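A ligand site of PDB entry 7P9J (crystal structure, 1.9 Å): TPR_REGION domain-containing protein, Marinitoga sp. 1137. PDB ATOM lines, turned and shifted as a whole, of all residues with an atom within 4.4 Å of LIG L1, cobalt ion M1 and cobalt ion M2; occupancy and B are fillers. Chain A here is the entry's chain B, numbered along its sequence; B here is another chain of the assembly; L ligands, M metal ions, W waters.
Of the 15 residues printed, 3 come within 4 Å of cobalt ion M2.
Water W2 lies within hydrogen-bond range of ND2 of Asn 165 (2.7 Å), N5 of LIG L1 (3.0 Å) and O10 of LG2 L2 (3.1 Å).
Cobalt ion M1 is bound by the side-chain carboxylate (OD1) of Asp 70 (2.2 Å), an oxygen (O1) of LG2 L2 (2.3 Å), an oxygen (O5) of LG2 L2 (2.3 Å), an oxygen (O3) of LG2 L2 (2.3 Å), the side-chain carboxylate (OD1) of Asp 68 (2.3 Å) and water W1 (2.5 Å).
Cobalt ion M2 is bound by OD2 of Asp 68, OE2 of Glu 151, O12 of LIG L1, O1 of LG2 L2 and OD2 of Asp 70.
Two residues have an atom within 4 Å of cobalt ion M1: Asp 68 and Asp 70. The nearest printed residue that does not touch cobalt ion M1 is Arg 114 (4.1 Å).
OH of Tyr 75 touches O3 of LIG L1, 3.9 Å away. Lys 155 touches LIG L1 (NZ to O11, 3.97 Å). Ten residues have an atom within 4 Å of LIG L1: Asp 70, Lys 72, Lys 73, Tyr 75, Arg 114, Glu 151, Lys 155, Asn 165, DC 7 of chain B and DA 8 of chain B. The nearest printed residue that does not touch LIG L1 is DT 6 of chain B (4.04 Å).
The side-chain amide oxygen of Asn 165 sits close to O3' of DA 8 of chain B. OE1 of Glu 151 lies within salt-bridge range of NZ of Lys 155 (3.5 Å). The side-chain amino group (NZ) of Lys 72 lies within salt-bridge range of the side-chain carboxylate (OD1) of Asp 149 (3.5 Å). The guanidinium group (NH2) of Arg 114 lies close to the side-chain carboxylate (OD2) of Asp 70, at 3.1 Å. O of Asp 70 sits at hydrogen-bond distance from N of Asp 149, at 2.7 Å. The side-chain carboxylate (OD1) of Asp 68 lies close to a ring nitrogen (NE2) of His 117, at 3.4 Å.
N3 of DA 8 of chain B sits close to N3 of LIG L1. A ring nitrogen (NE2) of His 117 lies close to an oxygen (O5) of LG2 L2, at 2.8 Å. The backbone NH (N) of Arg 114 is in hydrogen-bond range of an oxygen (O6) of LG2 L2. A nitrogen (N3) of LG2 L2 sits at hydrogen-bond distance from O4 of DT 6 of chain B (2.9 Å). An oxygen (O2) of LIG L1 sits at hydrogen-bond distance from the backbone NH (N) of Lys 73 (3.5 Å). The side-chain amide nitrogen (ND2) of Asn 165 sits close to a nitrogen (N4) of LIG L1 (3.4 Å). O4 of LG2 L2 lies within salt-bridge range of NH2 of Arg 114 (3.1 Å). O2 of DC 7 of chain B lies within hydrogen-bond range of a nitrogen (N4) of LIG L1, 2.9 Å away. An oxygen (O2) of LIG L1 lies within salt-bridge range of the guanidinium group (NH1) of Arg 114, 3.0 Å away. The side-chain amino group of Lys 72 lies within salt-bridge range of an oxygen (O6) of LIG L1, at 2.9 Å.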
ATOM      1  N   ASP A  68      -8.811 -21.620 -10.779  1.00  0.00           N
ATOM      2  CA  ASP A  68      -7.529 -22.229 -10.434  1.00  0.00           C
ATOM      3  C   ASP A  68      -6.821 -21.453  -9.313  1.00  0.00           C
ATOM      4  O   ASP A  68      -6.213 -20.402  -9.562  1.00  0.00           O
ATOM      5  CB  ASP A  68      -6.654 -22.326 -11.682  1.00  0.00           C
ATOM      6  CG  ASP A  68      -5.260 -22.839 -11.386  1.00  0.00           C
ATOM      7  OD1 ASP A  68      -5.120 -23.763 -10.543  1.00  0.00           O
ATOM      8  OD2 ASP A  68      -4.313 -22.355 -12.038  1.00  0.00           O
ATOM      9  N   ASP A  70      -3.870 -21.093  -6.755  1.00  0.00           N
ATOM     10  CA  ASP A  70      -2.472 -21.496  -6.736  1.00  0.00           C
ATOM     11  C   ASP A  70      -1.776 -20.882  -5.521  1.00  0.00           C
ATOM     12  O   ASP A  70      -1.851 -19.675  -5.312  1.00  0.00           O
ATOM     13  CB  ASP A  70      -1.765 -20.983  -7.988  1.00  0.00           C
ATOM     14  CG  ASP A  70      -1.897 -21.905  -9.159  1.00  0.00           C
ATOM     15  OD1 ASP A  70      -2.863 -22.694  -9.218  1.00  0.00           O
ATOM     16  OD2 ASP A  70      -1.066 -21.769 -10.071  1.00  0.00           O
ATOM     17  N   LYS A  72       1.508 -19.644  -4.715  1.00  0.00           N
ATOM     18  CA  LYS A  72       2.693 -19.212  -5.482  1.00  0.00           C
ATOM     19  C   LYS A  72       4.003 -19.690  -4.834  1.00  0.00           C
ATOM     20  O   LYS A  72       3.950 -20.220  -3.711  1.00  0.00           O
ATOM     21  CB  LYS A  72       2.675 -17.700  -5.657  1.00  0.00           C
ATOM     22  CG  LYS A  72       1.788 -17.186  -6.778  1.00  0.00           C
ATOM     23  CD  LYS A  72       1.656 -18.138  -7.950  1.00  0.00           C
ATOM     24  CE  LYS A  72       1.786 -17.468  -9.293  1.00  0.00           C
ATOM     25  NZ  LYS A  72       0.908 -18.090 -10.313  1.00  0.00           N
ATOM     26  N   LYS A  73       5.122 -19.473  -5.522  1.00  0.00           N
ATOM     27  CA  LYS A  73       6.470 -19.902  -5.065  1.00  0.00           C
ATOM     28  C   LYS A  73       6.705 -19.791  -3.548  1.00  0.00           C
ATOM     29  O   LYS A  73       7.075 -18.683  -3.096  1.00  0.00           O
ATOM     30  CB  LYS A  73       7.486 -18.995  -5.778  1.00  0.00           C
ATOM     31  N   TYR A  75       8.942 -22.036  -2.003  1.00  0.00           N
ATOM     32  CA  TYR A  75      10.413 -22.297  -2.048  1.00  0.00           C
ATOM     33  C   TYR A  75      10.964 -22.650  -0.668  1.00  0.00           C
ATOM     34  O   TYR A  75      10.805 -23.808  -0.238  1.00  0.00           O
ATOM     35  CB  TYR A  75      11.191 -21.118  -2.657  1.00  0.00           C
ATOM     36  CG  TYR A  75      10.990 -20.856  -4.128  1.00  0.00           C
ATOM     37  CD1 TYR A  75      10.357 -21.779  -4.949  1.00  0.00           C
ATOM     38  CD2 TYR A  75      11.437 -19.685  -4.700  1.00  0.00           C
ATOM     39  CE1 TYR A  75      10.180 -21.527  -6.300  1.00  0.00           C
ATOM     40  CE2 TYR A  75      11.276 -19.420  -6.044  1.00  0.00           C
ATOM     41  CZ  TYR A  75      10.643 -20.343  -6.851  1.00  0.00           C
ATOM     42  OH  TYR A  75      10.472 -20.081  -8.180  1.00  0.00           O
ATOM     43  N   ARG A 114      -0.225 -27.995  -5.729  1.00  0.00           N
ATOM     44  CA  ARG A 114      -0.277 -26.758  -4.919  1.00  0.00           C
ATOM     45  C   ARG A 114      -1.619 -26.036  -4.934  1.00  0.00           C
ATOM     46  O   ARG A 114      -1.627 -24.798  -4.915  1.00  0.00           O
ATOM     47  CB  ARG A 114       0.817 -25.809  -5.426  1.00  0.00           C
ATOM     48  CG  ARG A 114       0.846 -25.608  -6.934  1.00  0.00           C
ATOM     49  CD  ARG A 114       0.747 -24.156  -7.330  1.00  0.00           C
ATOM     50  NE  ARG A 114       0.802 -23.997  -8.774  1.00  0.00           N
ATOM     51  CZ  ARG A 114       1.635 -23.200  -9.412  1.00  0.00           C
ATOM     52  NH1 ARG A 114       2.490 -22.451  -8.740  1.00  0.00           N
ATOM     53  NH2 ARG A 114       1.606 -23.133 -10.729  1.00  0.00           N
ATOM     54  N   HIS A 117      -8.861 -26.691  -7.771  1.00  0.00           N
ATOM     55  CA  HIS A 117      -9.715 -26.208  -8.849  1.00  0.00           C
ATOM     56  C   HIS A 117     -11.157 -26.200  -8.347  1.00  0.00           C
ATOM     57  O   HIS A 117     -11.592 -27.135  -7.664  1.00  0.00           O
ATOM     58  CB  HIS A 117      -9.631 -27.106 -10.087  1.00  0.00           C
ATOM     59  CG  HIS A 117      -8.288 -27.127 -10.760  1.00  0.00           C
ATOM     60  ND1 HIS A 117      -7.860 -28.205 -11.502  1.00  0.00           N
ATOM     61  CD2 HIS A 117      -7.282 -26.218 -10.816  1.00  0.00           C
ATOM     62  CE1 HIS A 117      -6.642 -27.975 -11.975  1.00  0.00           C
ATOM     63  NE2 HIS A 117      -6.276 -26.771 -11.574  1.00  0.00           N
ATOM     64  N   ASP A 149      -2.662 -17.130  -5.785  1.00  0.00           N
ATOM     65  CA  ASP A 149      -3.031 -16.559  -7.102  1.00  0.00           C
ATOM     66  C   ASP A 149      -4.353 -17.199  -7.516  1.00  0.00           C
ATOM     67  O   ASP A 149      -4.559 -18.370  -7.193  1.00  0.00           O
ATOM     68  CB  ASP A 149      -1.913 -16.790  -8.123  1.00  0.00           C
ATOM     69  CG  ASP A 149      -2.361 -17.127  -9.535  1.00  0.00           C
ATOM     70  OD1 ASP A 149      -2.537 -18.322  -9.827  1.00  0.00           O
ATOM     71  OD2 ASP A 149      -2.521 -16.180 -10.336  1.00  0.00           O
ATOM     72  N   GLU A 151      -6.666 -17.969 -10.911  1.00  0.00           N
ATOM     73  CA  GLU A 151      -6.767 -17.903 -12.385  1.00  0.00           C
ATOM     74  C   GLU A 151      -8.172 -18.334 -12.804  1.00  0.00           C
ATOM     75  O   GLU A 151      -8.776 -19.168 -12.126  1.00  0.00           O
ATOM     76  CB  GLU A 151      -5.688 -18.752 -13.032  1.00  0.00           C
ATOM     77  CG  GLU A 151      -4.328 -18.112 -13.034  1.00  0.00           C
ATOM     78  CD  GLU A 151      -3.249 -19.077 -13.467  1.00  0.00           C
ATOM     79  OE1 GLU A 151      -3.116 -19.286 -14.685  1.00  0.00           O
ATOM     80  OE2 GLU A 151      -2.577 -19.637 -12.591  1.00  0.00           O
ATOM     81  N   PHE A 153     -10.440 -20.014 -15.840  1.00  0.00           N
ATOM     82  CA  PHE A 153     -10.495 -20.778 -17.090  1.00  0.00           C
ATOM     83  C   PHE A 153     -11.951 -20.833 -17.543  1.00  0.00           C
ATOM     84  O   PHE A 153     -12.784 -21.338 -16.782  1.00  0.00           O
ATOM     85  CB  PHE A 153      -9.956 -22.195 -16.870  1.00  0.00           C
ATOM     86  CG  PHE A 153      -8.466 -22.263 -16.776  1.00  0.00           C
ATOM     87  CD1 PHE A 153      -7.823 -21.922 -15.593  1.00  0.00           C
ATOM     88  CD2 PHE A 153      -7.693 -22.679 -17.858  1.00  0.00           C
ATOM     89  CE1 PHE A 153      -6.453 -21.961 -15.488  1.00  0.00           C
ATOM     90  CE2 PHE A 153      -6.316 -22.708 -17.760  1.00  0.00           C
ATOM     91  CZ  PHE A 153      -5.697 -22.360 -16.564  1.00  0.00           C
ATOM     92  N   LYS A 155      -9.463 -18.737 -20.258  1.00  0.00           N
ATOM     93  CA  LYS A 155      -8.503 -17.632 -20.260  1.00  0.00           C
ATOM     94  C   LYS A 155      -8.683 -16.701 -21.457  1.00  0.00           C
ATOM     95  O   LYS A 155      -8.022 -15.656 -21.522  1.00  0.00           O
ATOM     96  CB  LYS A 155      -7.073 -18.197 -20.246  1.00  0.00           C
ATOM     97  CG  LYS A 155      -6.595 -18.610 -18.866  1.00  0.00           C
ATOM     98  CD  LYS A 155      -5.092 -18.848 -18.790  1.00  0.00           C
ATOM     99  CE  LYS A 155      -4.413 -17.829 -17.885  1.00  0.00           C
ATOM    100  NZ  LYS A 155      -2.930 -17.902 -17.932  1.00  0.00           N
ATOM    101  N   ASN A 165      -6.779 -22.174 -24.170  1.00  0.00           N
ATOM    102  CA  ASN A 165      -6.076 -22.738 -23.031  1.00  0.00           C
ATOM    103  C   ASN A 165      -6.789 -23.993 -22.541  1.00  0.00           C
ATOM    104  O   ASN A 165      -8.001 -24.135 -22.698  1.00  0.00           O
ATOM    105  CB  ASN A 165      -5.939 -21.716 -21.896  1.00  0.00           C
ATOM    106  CG  ASN A 165      -4.742 -20.795 -22.089  1.00  0.00           C
ATOM    107  OD1 ASN A 165      -4.818 -19.821 -22.825  1.00  0.00           O
ATOM    108  ND2 ASN A 165      -3.639 -21.104 -21.427  1.00  0.00           N
ATOM    109  P    DT B   6       7.616 -28.336 -29.065  1.00  0.00           P
ATOM    110  OP1  DT B   6       8.413 -28.563 -30.291  1.00  0.00           O
ATOM    111  OP2  DT B   6       8.130 -27.448 -27.999  1.00  0.00           O
ATOM    112  O5'  DT B   6       6.180 -27.820 -29.511  1.00  0.00           O
ATOM    113  C5'  DT B   6       5.166 -28.749 -29.901  1.00  0.00           C
ATOM    114  C4'  DT B   6       3.799 -28.219 -29.525  1.00  0.00           C
ATOM    115  O4'  DT B   6       3.634 -28.239 -28.085  1.00  0.00           O
ATOM    116  C3'  DT B   6       3.513 -26.782 -29.967  1.00  0.00           C
ATOM    117  O3'  DT B   6       2.216 -26.747 -30.573  1.00  0.00           O
ATOM    118  C2'  DT B   6       3.575 -25.984 -28.674  1.00  0.00           C
ATOM    119  C1'  DT B   6       3.125 -27.001 -27.645  1.00  0.00           C
ATOM    120  N1   DT B   6       3.634 -26.763 -26.287  1.00  0.00           N
ATOM    121  C2   DT B   6       2.737 -26.520 -25.275  1.00  0.00           C
ATOM    122  O2   DT B   6       1.529 -26.479 -25.448  1.00  0.00           O
ATOM    123  N3   DT B   6       3.308 -26.351 -24.042  1.00  0.00           N
ATOM    124  C4   DT B   6       4.650 -26.381 -23.725  1.00  0.00           C
ATOM    125  O4   DT B   6       5.013 -26.198 -22.574  1.00  0.00           O
ATOM    126  C5   DT B   6       5.534 -26.640 -24.843  1.00  0.00           C
ATOM    127  C7   DT B   6       7.015 -26.693 -24.593  1.00  0.00           C
ATOM    128  C6   DT B   6       4.986 -26.814 -26.047  1.00  0.00           C
ATOM    129  P    DC B   7       1.803 -25.538 -31.509  1.00  0.00           P
ATOM    130  OP1  DC B   7       0.811 -26.037 -32.492  1.00  0.00           O
ATOM    131  OP2  DC B   7       3.025 -24.857 -31.982  1.00  0.00           O
ATOM    132  O5'  DC B   7       1.015 -24.567 -30.519  1.00  0.00           O
ATOM    133  C5'  DC B   7      -0.092 -25.059 -29.750  1.00  0.00           C
ATOM    134  C4'  DC B   7      -0.462 -24.088 -28.652  1.00  0.00           C
ATOM    135  O4'  DC B   7       0.474 -24.210 -27.557  1.00  0.00           O
ATOM    136  C3'  DC B   7      -0.438 -22.618 -29.074  1.00  0.00           C
ATOM    137  O3'  DC B   7      -1.757 -22.096 -28.902  1.00  0.00           O
ATOM    138  C2'  DC B   7       0.573 -21.975 -28.122  1.00  0.00           C
ATOM    139  C1'  DC B   7       0.607 -22.942 -26.963  1.00  0.00           C
ATOM    140  N1   DC B   7       1.851 -22.934 -26.188  1.00  0.00           N
ATOM    141  C2   DC B   7       1.764 -22.901 -24.797  1.00  0.00           C
ATOM    142  O2   DC B   7       0.651 -22.883 -24.261  1.00  0.00           O
ATOM    143  N3   DC B   7       2.903 -22.897 -24.060  1.00  0.00           N
ATOM    144  C4   DC B   7       4.094 -22.916 -24.680  1.00  0.00           C
ATOM    145  N4   DC B   7       5.187 -22.907 -23.922  1.00  0.00           N
ATOM    146  C5   DC B   7       4.205 -22.955 -26.099  1.00  0.00           C
ATOM    147  C6   DC B   7       3.069 -22.942 -26.807  1.00  0.00           C
ATOM    148  P    DA B   8      -2.142 -20.647 -29.438  1.00  0.00           P
ATOM    149  OP1  DA B   8      -3.507 -20.713 -29.959  1.00  0.00           O
ATOM    150  OP2  DA B   8      -1.053 -20.133 -30.293  1.00  0.00           O
ATOM    151  O5'  DA B   8      -2.223 -19.791 -28.100  1.00  0.00           O
ATOM    152  C5'  DA B   8      -3.145 -20.189 -27.073  1.00  0.00           C
ATOM    153  C4'  DA B   8      -2.703 -19.673 -25.720  1.00  0.00           C
ATOM    154  O4'  DA B   8      -1.417 -20.213 -25.383  1.00  0.00           O
ATOM    155  C3'  DA B   8      -2.529 -18.164 -25.659  1.00  0.00           C
ATOM    156  O3'  DA B   8      -3.770 -17.576 -25.260  1.00  0.00           O
ATOM    157  C2'  DA B   8      -1.471 -17.995 -24.579  1.00  0.00           C
ATOM    158  C1'  DA B   8      -0.749 -19.327 -24.498  1.00  0.00           C
ATOM    159  N9   DA B   8       0.661 -19.285 -24.887  1.00  0.00           N
ATOM    160  C8   DA B   8       1.187 -19.209 -26.151  1.00  0.00           C
ATOM    161  N7   DA B   8       2.489 -19.233 -26.188  1.00  0.00           N
ATOM    162  C5   DA B   8       2.858 -19.317 -24.850  1.00  0.00           C
ATOM    163  C6   DA B   8       4.101 -19.380 -24.209  1.00  0.00           C
ATOM    164  N6   DA B   8       5.268 -19.341 -24.866  1.00  0.00           N
ATOM    165  N1   DA B   8       4.116 -19.468 -22.864  1.00  0.00           N
ATOM    166  C2   DA B   8       2.950 -19.484 -22.215  1.00  0.00           C
ATOM    167  N3   DA B   8       1.715 -19.444 -22.700  1.00  0.00           N
ATOM    168  C4   DA B   8       1.733 -19.359 -24.045  1.00  0.00           C
HETATM  169  P1  LIG L   1       5.423 -19.372  -9.669  1.00  0.00           P
HETATM  170  O1  LIG L   1       5.232 -17.932  -9.282  1.00  0.00           O
HETATM  171  O2  LIG L   1       4.598 -20.306  -8.839  1.00  0.00           O
HETATM  172  O3  LIG L   1       6.871 -19.764  -9.713  1.00  0.00           O
HETATM  173  O4  LIG L   1       4.896 -19.506 -11.192  1.00  0.00           O
HETATM  174  P2  LIG L   1       3.891 -20.499 -11.920  1.00  0.00           P
HETATM  175  O5  LIG L   1       4.480 -21.871 -11.926  1.00  0.00           O
HETATM  176  O6  LIG L   1       2.524 -20.301 -11.370  1.00  0.00           O
HETATM  177  O7  LIG L   1       3.908 -19.945 -13.412  1.00  0.00           O
HETATM  178  P3  LIG L   1       3.783 -18.471 -14.014  1.00  0.00           P
HETATM  179  O8  LIG L   1       3.521 -17.501 -12.914  1.00  0.00           O
HETATM  180  O9  LIG L   1       4.949 -18.231 -14.906  1.00  0.00           O
HETATM  181  O10 LIG L   1       2.466 -18.617 -14.915  1.00  0.00           O
HETATM  182  C1  LIG L   1       1.169 -18.412 -14.286  1.00  0.00           C
HETATM  183  C2  LIG L   1       0.196 -19.463 -14.773  1.00  0.00           C
HETATM  184  O11 LIG L   1       0.253 -19.554 -16.220  1.00  0.00           O
HETATM  185  C3  LIG L   1       0.423 -20.892 -14.276  1.00  0.00           C
HETATM  186  O12 LIG L   1      -0.169 -21.101 -12.997  1.00  0.00           O
HETATM  187  C4  LIG L   1      -0.275 -21.695 -15.368  1.00  0.00           C
HETATM  188  O13 LIG L   1      -1.674 -21.700 -15.212  1.00  0.00           O
HETATM  189  C5  LIG L   1       0.037 -20.889 -16.625  1.00  0.00           C
HETATM  190  N1  LIG L   1       1.209 -21.345 -17.380  1.00  0.00           N
HETATM  191  C6  LIG L   1       2.498 -21.493 -16.928  1.00  0.00           C
HETATM  192  N2  LIG L   1       3.320 -21.901 -17.854  1.00  0.00           N
HETATM  193  C7  LIG L   1       2.535 -22.024 -18.986  1.00  0.00           C
HETATM  194  C8  LIG L   1       2.876 -22.426 -20.297  1.00  0.00           C
HETATM  195  O14 LIG L   1       3.992 -22.752 -20.737  1.00  0.00           O
HETATM  196  N3  LIG L   1       1.767 -22.420 -21.146  1.00  0.00           N
HETATM  197  C9  LIG L   1       0.497 -22.057 -20.773  1.00  0.00           C
HETATM  198  N4  LIG L   1      -0.435 -22.112 -21.725  1.00  0.00           N
HETATM  199  N5  LIG L   1       0.169 -21.682 -19.547  1.00  0.00           N
HETATM  200  C10 LIG L   1       1.224 -21.687 -18.705  1.00  0.00           C
HETATM  201  N1  LG2 L   2       1.170 -25.743 -21.681  1.00  0.00           N
HETATM  202  C1  LG2 L   2      -0.176 -25.739 -21.729  1.00  0.00           C
HETATM  203  N2  LG2 L   2      -1.063 -25.659 -20.715  1.00  0.00           N
HETATM  204  C2  LG2 L   2      -0.416 -25.568 -19.564  1.00  0.00           C
HETATM  205  C3  LG2 L   2       0.979 -25.565 -19.388  1.00  0.00           C
HETATM  206  C4  LG2 L   2       1.722 -25.659 -20.504  1.00  0.00           C
HETATM  207  N3  LG2 L   2       3.161 -25.655 -20.369  1.00  0.00           N
HETATM  208  N4  LG2 L   2       1.274 -25.440 -17.906  1.00  0.00           N
HETATM  209  C5  LG2 L   2       0.021 -25.395 -17.408  1.00  0.00           C
HETATM  210  N5  LG2 L   2      -0.828 -25.471 -18.364  1.00  0.00           N
HETATM  211  P1  LG2 L   2      -1.058 -24.921 -13.170  1.00  0.00           P
HETATM  212  P2  LG2 L   2      -2.486 -27.323 -12.149  1.00  0.00           P
HETATM  213  P3  LG2 L   2      -1.000 -27.360  -9.749  1.00  0.00           P
HETATM  214  C6  LG2 L   2      -2.220 -25.471 -18.123  1.00  0.00           C
HETATM  215  O1  LG2 L   2      -1.590 -24.112 -12.095  1.00  0.00           O
HETATM  216  O2  LG2 L   2      -3.228 -28.185 -13.029  1.00  0.00           O
HETATM  217  O3  LG2 L   2      -1.094 -25.930  -9.805  1.00  0.00           O
HETATM  218  C7  LG2 L   2      -2.598 -26.866 -17.610  1.00  0.00           C
HETATM  219  O4  LG2 L   2       0.332 -24.520 -13.162  1.00  0.00           O
HETATM  220  O5  LG2 L   2      -3.470 -26.352 -11.771  1.00  0.00           O
HETATM  221  O6  LG2 L   2      -1.307 -27.666  -8.379  1.00  0.00           O
HETATM  222  C8  LG2 L   2      -2.923 -26.615 -16.191  1.00  0.00           C
HETATM  223  O7  LG2 L   2      -3.890 -27.530 -15.696  1.00  0.00           O
HETATM  224  N6  LG2 L   2      -1.161 -26.592 -12.917  1.00  0.00           N
HETATM  225  O8  LG2 L   2      -1.949 -28.125 -10.833  1.00  0.00           O
HETATM  226  O9  LG2 L   2       0.409 -27.624  -9.859  1.00  0.00           O
HETATM  227  C9  LG2 L   2      -3.405 -25.215 -16.141  1.00  0.00           C
HETATM  228  O10 LG2 L   2      -2.690 -24.488 -17.148  1.00  0.00           O
HETATM  229  C10 LG2 L   2      -3.112 -24.651 -14.764  1.00  0.00           C
HETATM  230  O11 LG2 L   2      -1.739 -24.536 -14.603  1.00  0.00           O
HETATM  231 CO    CO M   1      -2.954 -24.617 -10.333  1.00  0.00          CO
HETATM  232 CO    CO M   2      -2.180 -21.838 -12.207  1.00  0.00          CO
HETATM  233  O   HOH W   1      -4.380 -25.671  -8.530  1.00  0.00           O
HETATM  234  O   HOH W   2      -2.802 -22.053 -19.014  1.00  0.00           O
